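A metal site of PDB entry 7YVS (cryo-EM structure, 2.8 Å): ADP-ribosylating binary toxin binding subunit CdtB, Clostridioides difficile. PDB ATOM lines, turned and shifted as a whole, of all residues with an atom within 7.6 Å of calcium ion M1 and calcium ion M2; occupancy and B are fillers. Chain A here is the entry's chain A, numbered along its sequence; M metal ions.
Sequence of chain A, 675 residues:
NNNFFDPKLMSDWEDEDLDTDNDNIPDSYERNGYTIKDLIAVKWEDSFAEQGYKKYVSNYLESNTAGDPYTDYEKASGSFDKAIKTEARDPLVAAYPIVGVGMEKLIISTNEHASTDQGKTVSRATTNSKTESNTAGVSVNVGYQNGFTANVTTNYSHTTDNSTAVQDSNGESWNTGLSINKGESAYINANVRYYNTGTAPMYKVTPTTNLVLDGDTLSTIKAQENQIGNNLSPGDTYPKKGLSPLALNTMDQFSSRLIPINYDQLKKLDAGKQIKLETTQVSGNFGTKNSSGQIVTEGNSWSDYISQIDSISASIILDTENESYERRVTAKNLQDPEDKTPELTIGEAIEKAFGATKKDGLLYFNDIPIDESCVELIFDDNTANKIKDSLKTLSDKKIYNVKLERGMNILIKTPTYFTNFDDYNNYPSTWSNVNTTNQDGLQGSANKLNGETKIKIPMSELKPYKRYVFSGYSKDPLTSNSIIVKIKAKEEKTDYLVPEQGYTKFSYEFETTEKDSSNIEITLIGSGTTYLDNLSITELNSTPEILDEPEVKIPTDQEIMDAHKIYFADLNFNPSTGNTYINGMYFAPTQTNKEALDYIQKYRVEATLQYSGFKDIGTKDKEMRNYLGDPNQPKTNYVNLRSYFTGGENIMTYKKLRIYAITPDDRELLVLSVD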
ATOM      1  N   LEU A  18      10.654 -25.091  20.857  1.00  0.00           N
ATOM      2  CA  LEU A  18      10.776 -24.450  19.551  1.00  0.00           C
ATOM      3  C   LEU A  18      12.154 -23.799  19.437  1.00  0.00           C
ATOM      4  O   LEU A  18      12.541 -23.009  20.309  1.00  0.00           O
ATOM      5  CB  LEU A  18       9.675 -23.403  19.363  1.00  0.00           C
ATOM      6  CG  LEU A  18       9.612 -22.657  18.040  1.00  0.00           C
ATOM      7  CD1 LEU A  18       9.413 -23.616  16.885  1.00  0.00           C
ATOM      8  CD2 LEU A  18       8.482 -21.649  18.081  1.00  0.00           C
ATOM      9  N   ASP A  19      12.881 -24.135  18.375  1.00  0.00           N
ATOM     10  CA  ASP A  19      14.261 -23.685  18.177  1.00  0.00           C
ATOM     11  C   ASP A  19      14.353 -23.056  16.796  1.00  0.00           C
ATOM     12  O   ASP A  19      14.550 -23.763  15.799  1.00  0.00           O
ATOM     13  CB  ASP A  19      15.226 -24.842  18.340  1.00  0.00           C
ATOM     14  CG  ASP A  19      16.635 -24.397  18.603  1.00  0.00           C
ATOM     15  OD1 ASP A  19      16.857 -23.172  18.719  1.00  0.00           O
ATOM     16  OD2 ASP A  19      17.528 -25.257  18.700  1.00  0.00           O
ATOM     17  N   THR A  20      14.226 -21.738  16.730  1.00  0.00           N
ATOM     18  CA  THR A  20      14.198 -21.043  15.441  1.00  0.00           C
ATOM     19  C   THR A  20      15.584 -21.019  14.789  1.00  0.00           C
ATOM     20  O   THR A  20      15.712 -21.272  13.588  1.00  0.00           O
ATOM     21  CB  THR A  20      13.662 -19.628  15.612  1.00  0.00           C
ATOM     22  OG1 THR A  20      12.407 -19.679  16.317  1.00  0.00           O
ATOM     23  CG2 THR A  20      13.437 -18.970  14.267  1.00  0.00           C
ATOM     24  N   ASP A  21      16.616 -20.707  15.564  1.00  0.00           N
ATOM     25  CA  ASP A  21      17.951 -20.572  14.994  1.00  0.00           C
ATOM     26  C   ASP A  21      18.737 -21.871  14.957  1.00  0.00           C
ATOM     27  O   ASP A  21      19.850 -21.881  14.427  1.00  0.00           O
ATOM     28  CB  ASP A  21      18.756 -19.520  15.772  1.00  0.00           C
ATOM     29  CG  ASP A  21      18.634 -19.695  17.259  1.00  0.00           C
ATOM     30  OD1 ASP A  21      17.865 -20.570  17.690  1.00  0.00           O
ATOM     31  OD2 ASP A  21      19.310 -18.949  17.994  1.00  0.00           O
ATOM     32  N   ASN A  22      18.191 -22.949  15.516  1.00  0.00           N
ATOM     33  CA  ASN A  22      18.829 -24.268  15.512  1.00  0.00           C
ATOM     34  C   ASN A  22      20.192 -24.238  16.204  1.00  0.00           C
ATOM     35  O   ASN A  22      21.231 -24.535  15.614  1.00  0.00           O
ATOM     36  CB  ASN A  22      18.957 -24.800  14.075  1.00  0.00           C
ATOM     37  CG  ASN A  22      17.625 -25.172  13.468  1.00  0.00           C
ATOM     38  OD1 ASN A  22      16.908 -26.018  13.987  1.00  0.00           O
ATOM     39  ND2 ASN A  22      17.298 -24.538  12.346  1.00  0.00           N
ATOM     40  N   ASP A  23      20.168 -23.874  17.493  1.00  0.00           N
ATOM     41  CA  ASP A  23      21.370 -23.948  18.321  1.00  0.00           C
ATOM     42  C   ASP A  23      21.127 -24.757  19.589  1.00  0.00           C
ATOM     43  O   ASP A  23      21.800 -24.519  20.598  1.00  0.00           O
ATOM     44  CB  ASP A  23      21.882 -22.552  18.668  1.00  0.00           C
ATOM     45  CG  ASP A  23      20.829 -21.690  19.328  1.00  0.00           C
ATOM     46  OD1 ASP A  23      19.655 -22.103  19.372  1.00  0.00           O
ATOM     47  OD2 ASP A  23      21.192 -20.594  19.802  1.00  0.00           O
ATOM     48  N   ASN A  24      20.166 -25.682  19.573  1.00  0.00           N
ATOM     49  CA  ASN A  24      19.891 -26.600  20.669  1.00  0.00           C
ATOM     50  C   ASN A  24      19.360 -25.892  21.914  1.00  0.00           C
ATOM     51  O   ASN A  24      19.308 -26.500  22.991  1.00  0.00           O
ATOM     52  CB  ASN A  24      21.122 -27.426  21.029  1.00  0.00           C
ATOM     53  CG  ASN A  24      21.679 -28.188  19.847  1.00  0.00           C
ATOM     54  OD1 ASN A  24      21.094 -28.192  18.762  1.00  0.00           O
ATOM     55  ND2 ASN A  24      22.820 -28.831  20.041  1.00  0.00           N
ATOM     56  N   ILE A  25      18.955 -24.637  21.799  1.00  0.00           N
ATOM     57  CA  ILE A  25      18.350 -23.924  22.924  1.00  0.00           C
ATOM     58  C   ILE A  25      16.976 -23.439  22.502  1.00  0.00           C
ATOM     59  O   ILE A  25      16.853 -22.737  21.492  1.00  0.00           O
ATOM     60  CB  ILE A  25      19.228 -22.758  23.400  1.00  0.00           C
ATOM     61  CG1 ILE A  25      20.691 -23.174  23.471  1.00  0.00           C
ATOM     62  CG2 ILE A  25      18.784 -22.287  24.763  1.00  0.00           C
ATOM     63  CD1 ILE A  25      21.639 -22.023  23.658  1.00  0.00           C
ATOM     64  N   PRO A  26      15.912 -23.788  23.231  1.00  0.00           N
ATOM     65  CA  PRO A  26      14.573 -23.333  22.845  1.00  0.00           C
ATOM     66  C   PRO A  26      14.444 -21.823  22.930  1.00  0.00           C
ATOM     67  O   PRO A  26      15.170 -21.158  23.667  1.00  0.00           O
ATOM     68  CB  PRO A  26      13.657 -24.033  23.857  1.00  0.00           C
ATOM     69  CG  PRO A  26      14.457 -25.186  24.358  1.00  0.00           C
ATOM     70  CD  PRO A  26      15.868 -24.727  24.360  1.00  0.00           C
ATOM     71  N   ASP A  27      13.499 -21.288  22.156  1.00  0.00           N
ATOM     72  CA  ASP A  27      13.330 -19.847  22.076  1.00  0.00           C
ATOM     73  C   ASP A  27      12.974 -19.241  23.424  1.00  0.00           C
ATOM     74  O   ASP A  27      13.523 -18.206  23.816  1.00  0.00           O
ATOM     75  CB  ASP A  27      12.256 -19.504  21.039  1.00  0.00           C
ATOM     76  CG  ASP A  27      12.709 -19.775  19.628  1.00  0.00           C
ATOM     77  OD1 ASP A  27      13.891 -20.131  19.434  1.00  0.00           O
ATOM     78  OD2 ASP A  27      11.889 -19.637  18.702  1.00  0.00           O
ATOM     79  N   SER A  28      12.054 -19.868  24.158  1.00  0.00           N
ATOM     80  CA  SER A  28      11.641 -19.324  25.442  1.00  0.00           C
ATOM     81  C   SER A  28      12.758 -19.370  26.465  1.00  0.00           C
ATOM     82  O   SER A  28      12.868 -18.465  27.300  1.00  0.00           O
ATOM     83  CB  SER A  28      10.407 -20.070  25.961  1.00  0.00           C
ATOM     84  OG  SER A  28      10.645 -21.465  26.030  1.00  0.00           O
ATOM     85  N   GLU A  30      16.018 -19.060  25.828  1.00  0.00           N
ATOM     86  CA  GLU A  30      16.888 -17.931  25.497  1.00  0.00           C
ATOM     87  C   GLU A  30      16.251 -16.614  25.909  1.00  0.00           C
ATOM     88  O   GLU A  30      16.928 -15.692  26.373  1.00  0.00           O
ATOM     89  CB  GLU A  30      17.191 -17.914  24.005  1.00  0.00           C
ATOM     90  CG  GLU A  30      17.923 -19.113  23.493  1.00  0.00           C
ATOM     91  CD  GLU A  30      18.593 -18.848  22.174  1.00  0.00           C
ATOM     92  OE1 GLU A  30      19.509 -18.004  22.128  1.00  0.00           O
ATOM     93  OE2 GLU A  30      18.213 -19.481  21.173  1.00  0.00           O
ATOM     94  N   TYR A  34      18.391 -19.299  31.076  1.00  0.00           N
ATOM     95  CA  TYR A  34      18.695 -20.726  31.085  1.00  0.00           C
ATOM     96  C   TYR A  34      20.090 -20.938  31.651  1.00  0.00           C
ATOM     97  O   TYR A  34      20.824 -19.991  31.927  1.00  0.00           O
ATOM     98  CB  TYR A  34      18.599 -21.331  29.672  1.00  0.00           C
ATOM     99  CG  TYR A  34      19.567 -20.740  28.682  1.00  0.00           C
ATOM    100  CD1 TYR A  34      19.279 -19.559  28.022  1.00  0.00           C
ATOM    101  CD2 TYR A  34      20.771 -21.363  28.389  1.00  0.00           C
ATOM    102  CE1 TYR A  34      20.158 -19.010  27.111  1.00  0.00           C
ATOM    103  CE2 TYR A  34      21.651 -20.828  27.489  1.00  0.00           C
ATOM    104  CZ  TYR A  34      21.340 -19.653  26.851  1.00  0.00           C
ATOM    105  OH  TYR A  34      22.211 -19.108  25.944  1.00  0.00           O
ATOM    106  N   SER A  58      20.155 -14.757  25.581  1.00  0.00           N
ATOM    107  CA  SER A  58      20.773 -14.609  24.270  1.00  0.00           C
ATOM    108  C   SER A  58      19.700 -14.310  23.230  1.00  0.00           C
ATOM    109  O   SER A  58      18.510 -14.244  23.544  1.00  0.00           O
ATOM    110  CB  SER A  58      21.565 -15.858  23.894  1.00  0.00           C
ATOM    111  OG  SER A  58      20.740 -17.007  23.880  1.00  0.00           O
ATOM    112  N   ASN A  59      20.148 -14.127  22.002  1.00  0.00           N
ATOM    113  CA  ASN A  59      19.269 -13.819  20.880  1.00  0.00           C
ATOM    114  C   ASN A  59      18.658 -15.113  20.355  1.00  0.00           C
ATOM    115  O   ASN A  59      19.377 -16.024  19.962  1.00  0.00           O
ATOM    116  CB  ASN A  59      20.049 -13.100  19.796  1.00  0.00           C
ATOM    117  CG  ASN A  59      19.166 -12.474  18.745  1.00  0.00           C
ATOM    118  OD1 ASN A  59      17.984 -12.787  18.640  1.00  0.00           O
ATOM    119  ND2 ASN A  59      19.733 -11.578  17.957  1.00  0.00           N
ATOM    120  N   TYR A  60      17.326 -15.189  20.337  1.00  0.00           N
ATOM    121  CA  TYR A  60      16.659 -16.394  19.883  1.00  0.00           C
ATOM    122  C   TYR A  60      16.510 -16.445  18.367  1.00  0.00           C
ATOM    123  O   TYR A  60      15.997 -17.449  17.855  1.00  0.00           O
ATOM    124  CB  TYR A  60      15.299 -16.550  20.556  1.00  0.00           C
ATOM    125  CG  TYR A  60      14.209 -15.638  20.047  1.00  0.00           C
ATOM    126  CD1 TYR A  60      14.087 -14.334  20.511  1.00  0.00           C
ATOM    127  CD2 TYR A  60      13.288 -16.078  19.111  1.00  0.00           C
ATOM    128  CE1 TYR A  60      13.085 -13.511  20.049  1.00  0.00           C
ATOM    129  CE2 TYR A  60      12.290 -15.263  18.647  1.00  0.00           C
ATOM    130  CZ  TYR A  60      12.194 -13.973  19.119  1.00  0.00           C
ATOM    131  OH  TYR A  60      11.192 -13.150  18.657  1.00  0.00           O
ATOM    132  N   LEU A  61      16.931 -15.411  17.656  1.00  0.00           N
ATOM    133  CA  LEU A  61      16.921 -15.395  16.196  1.00  0.00           C
ATOM    134  C   LEU A  61      18.324 -15.473  15.608  1.00  0.00           C
ATOM    135  O   LEU A  61      18.458 -15.568  14.380  1.00  0.00           O
ATOM    136  CB  LEU A  61      16.202 -14.148  15.692  1.00  0.00           C
ATOM    137  CG  LEU A  61      14.670 -14.197  15.738  1.00  0.00           C
ATOM    138  CD1 LEU A  61      14.080 -12.917  15.201  1.00  0.00           C
ATOM    139  CD2 LEU A  61      14.152 -15.384  14.966  1.00  0.00           C
ATOM    140  N   GLU A  62      19.361 -15.439  16.440  1.00  0.00           N
ATOM    141  CA  GLU A  62      20.743 -15.564  16.008  1.00  0.00           C
ATOM    142  C   GLU A  62      21.372 -16.770  16.688  1.00  0.00           C
ATOM    143  O   GLU A  62      21.192 -16.982  17.884  1.00  0.00           O
ATOM    144  CB  GLU A  62      21.553 -14.316  16.343  1.00  0.00           C
ATOM    145  CG  GLU A  62      21.409 -13.193  15.340  1.00  0.00           C
ATOM    146  CD  GLU A  62      22.136 -13.468  14.043  1.00  0.00           C
ATOM    147  OE1 GLU A  62      23.122 -14.243  14.073  1.00  0.00           O
ATOM    148  OE2 GLU A  62      21.724 -12.928  12.994  1.00  0.00           O
ATOM    149  N   SER A  63      22.121 -17.560  15.912  1.00  0.00           N
ATOM    150  CA  SER A  63      22.856 -18.681  16.473  1.00  0.00           C
ATOM    151  C   SER A  63      24.169 -18.235  17.107  1.00  0.00           C
ATOM    152  O   SER A  63      24.733 -18.965  17.924  1.00  0.00           O
ATOM    153  CB  SER A  63      23.114 -19.737  15.407  1.00  0.00           C
ATOM    154  OG  SER A  63      23.524 -20.945  16.000  1.00  0.00           O
ATOM    155  N   ASN A  64      24.674 -17.071  16.724  1.00  0.00           N
ATOM    156  CA  ASN A  64      25.884 -16.481  17.299  1.00  0.00           C
ATOM    157  C   ASN A  64      25.514 -15.062  17.734  1.00  0.00           C
ATOM    158  O   ASN A  64      25.611 -14.124  16.941  1.00  0.00           O
ATOM    159  CB  ASN A  64      27.033 -16.491  16.306  1.00  0.00           C
ATOM    160  CG  ASN A  64      27.414 -17.877  15.856  1.00  0.00           C
ATOM    161  OD1 ASN A  64      26.580 -18.635  15.375  1.00  0.00           O
ATOM    162  ND2 ASN A  64      28.685 -18.216  15.991  1.00  0.00           N
ATOM    163  N   THR A  65      25.096 -14.911  18.993  1.00  0.00           N
ATOM    164  CA  THR A  65      24.627 -13.616  19.461  1.00  0.00           C
ATOM    165  C   THR A  65      25.750 -12.584  19.477  1.00  0.00           C
ATOM    166  O   THR A  65      25.533 -11.420  19.118  1.00  0.00           O
ATOM    167  CB  THR A  65      24.023 -13.760  20.856  1.00  0.00           C
ATOM    168  OG1 THR A  65      23.004 -14.773  20.820  1.00  0.00           O
ATOM    169  CG2 THR A  65      23.405 -12.459  21.314  1.00  0.00           C
ATOM    170  N   THR A  71      28.965 -20.658  18.614  1.00  0.00           N
ATOM    171  CA  THR A  71      27.531 -20.482  18.771  1.00  0.00           C
ATOM    172  C   THR A  71      27.177 -20.243  20.240  1.00  0.00           C
ATOM    173  O   THR A  71      28.015 -20.351  21.136  1.00  0.00           O
ATOM    174  CB  THR A  71      26.769 -21.709  18.252  1.00  0.00           C
ATOM    175  OG1 THR A  71      26.833 -22.753  19.213  1.00  0.00           O
ATOM    176  CG2 THR A  71      27.365 -22.189  16.954  1.00  0.00           C
ATOM    177  N   ASP A  72      25.916 -19.889  20.476  1.00  0.00           N
ATOM    178  CA  ASP A  72      25.477 -19.633  21.845  1.00  0.00           C
ATOM    179  C   ASP A  72      25.587 -20.877  22.710  1.00  0.00           C
ATOM    180  O   ASP A  72      26.033 -20.804  23.852  1.00  0.00           O
ATOM    181  CB  ASP A  72      24.042 -19.109  21.833  1.00  0.00           C
ATOM    182  CG  ASP A  72      23.926 -17.741  21.184  1.00  0.00           C
ATOM    183  OD1 ASP A  72      24.953 -17.065  21.033  1.00  0.00           O
ATOM    184  OD2 ASP A  72      22.795 -17.351  20.830  1.00  0.00           O
ATOM    185  N   TYR A  73      25.188 -22.027  22.172  1.00  0.00           N
ATOM    186  CA  TYR A  73      25.286 -23.276  22.930  1.00  0.00           C
ATOM    187  C   TYR A  73      26.731 -23.648  23.197  1.00  0.00           C
ATOM    188  O   TYR A  73      27.065 -24.070  24.307  1.00  0.00           O
ATOM    189  CB  TYR A  73      24.586 -24.407  22.191  1.00  0.00           C
ATOM    190  CG  TYR A  73      24.769 -25.741  22.863  1.00  0.00           C
ATOM    191  CD1 TYR A  73      24.065 -26.078  24.002  1.00  0.00           C
ATOM    192  CD2 TYR A  73      25.672 -26.671  22.358  1.00  0.00           C
ATOM    193  CE1 TYR A  73      24.239 -27.296  24.619  1.00  0.00           C
ATOM    194  CE2 TYR A  73      25.855 -27.884  22.971  1.00  0.00           C
ATOM    195  CZ  TYR A  73      25.138 -28.189  24.096  1.00  0.00           C
ATOM    196  OH  TYR A  73      25.320 -29.402  24.709  1.00  0.00           O
ATOM    197  N   PRO A  91      26.821 -15.880  26.323  1.00  0.00           N
ATOM    198  CA  PRO A  91      26.602 -15.532  24.919  1.00  0.00           C
ATOM    199  C   PRO A  91      26.778 -14.052  24.587  1.00  0.00           C
ATOM    200  O   PRO A  91      26.981 -13.725  23.421  1.00  0.00           O
ATOM    201  CB  PRO A  91      25.161 -15.973  24.672  1.00  0.00           C
ATOM    202  CG  PRO A  91      24.913 -17.025  25.686  1.00  0.00           C
ATOM    203  CD  PRO A  91      25.661 -16.599  26.895  1.00  0.00           C
HETATM  204 CA    CA M   1      20.545 -18.125  19.903  1.00  0.00          CA
HETATM  205 CA    CA M   2      17.451 -21.193  19.836  1.00  0.00          CA
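Within 4 Å of calcium ion M1: Asp 21, Asp 23, Glu 30, Asn 59, Glu 62 and Asp 72.
The nearest printed residue that does not touch calcium ion M1 is Ser 58 (4.1 Å).
Asp 27 touches calcium ion M2 (OD1 to CA, 3.7 Å).
Calcium ion M2 is bound by the side-chain carboxylate of Asp 21 (2.3 Å), the side-chain carboxylate of Glu 30 (2.3 Å), the backbone carbonyl oxygen of Ile 25 (2.3 Å), the side-chain carboxylate of Asp 19 (2.3 Å) and the side-chain carboxylate of Asp 23 (2.4 Å).
Calcium ion M2 has five donor atoms within binding distance.
Calcium ion M1 is bound by O of Asn 59 (2.4 Å), O of Glu 62 (2.4 Å), OD2 of Asp 21 (2.4 Å), OE1 of Glu 30 (2.5 Å), OD2 of Asp 72 (2.6 Å) and OD2 of Asp 23 (2.6 Å).
Slightly farther from calcium ion M1 lies OE2 of Glu 30 (3.0 Å).
O of Glu 30 lies within hydrogen-bond range of N of Ser 58.
OD1 of Asp 19 lies close to N of Asn 22, at 3.5 Å.
O of Ser 63 sits at hydrogen-bond distance from N of Asp 72 (3.0 Å).
The side-chain carboxylate of Asp 27 lies within hydrogen-bond range of the side-chain hydroxyl of Thr 20 (2.4 Å).
The side-chain carboxylate of Asp 72 is in hydrogen-bond range of the backbone NH of Thr 65, at 3.0 Å.
OD1 of Asn 59 sits at hydrogen-bond distance from N of Leu 61 (3.0 Å).
O of Leu 18 is in hydrogen-bond range of N of Asp 27 (2.7 Å).
The side-chain carboxylate (OD2) of Asp 19 lies within hydrogen-bond range of the backbone NH (N) of Asn 24, 2.8 Å away.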
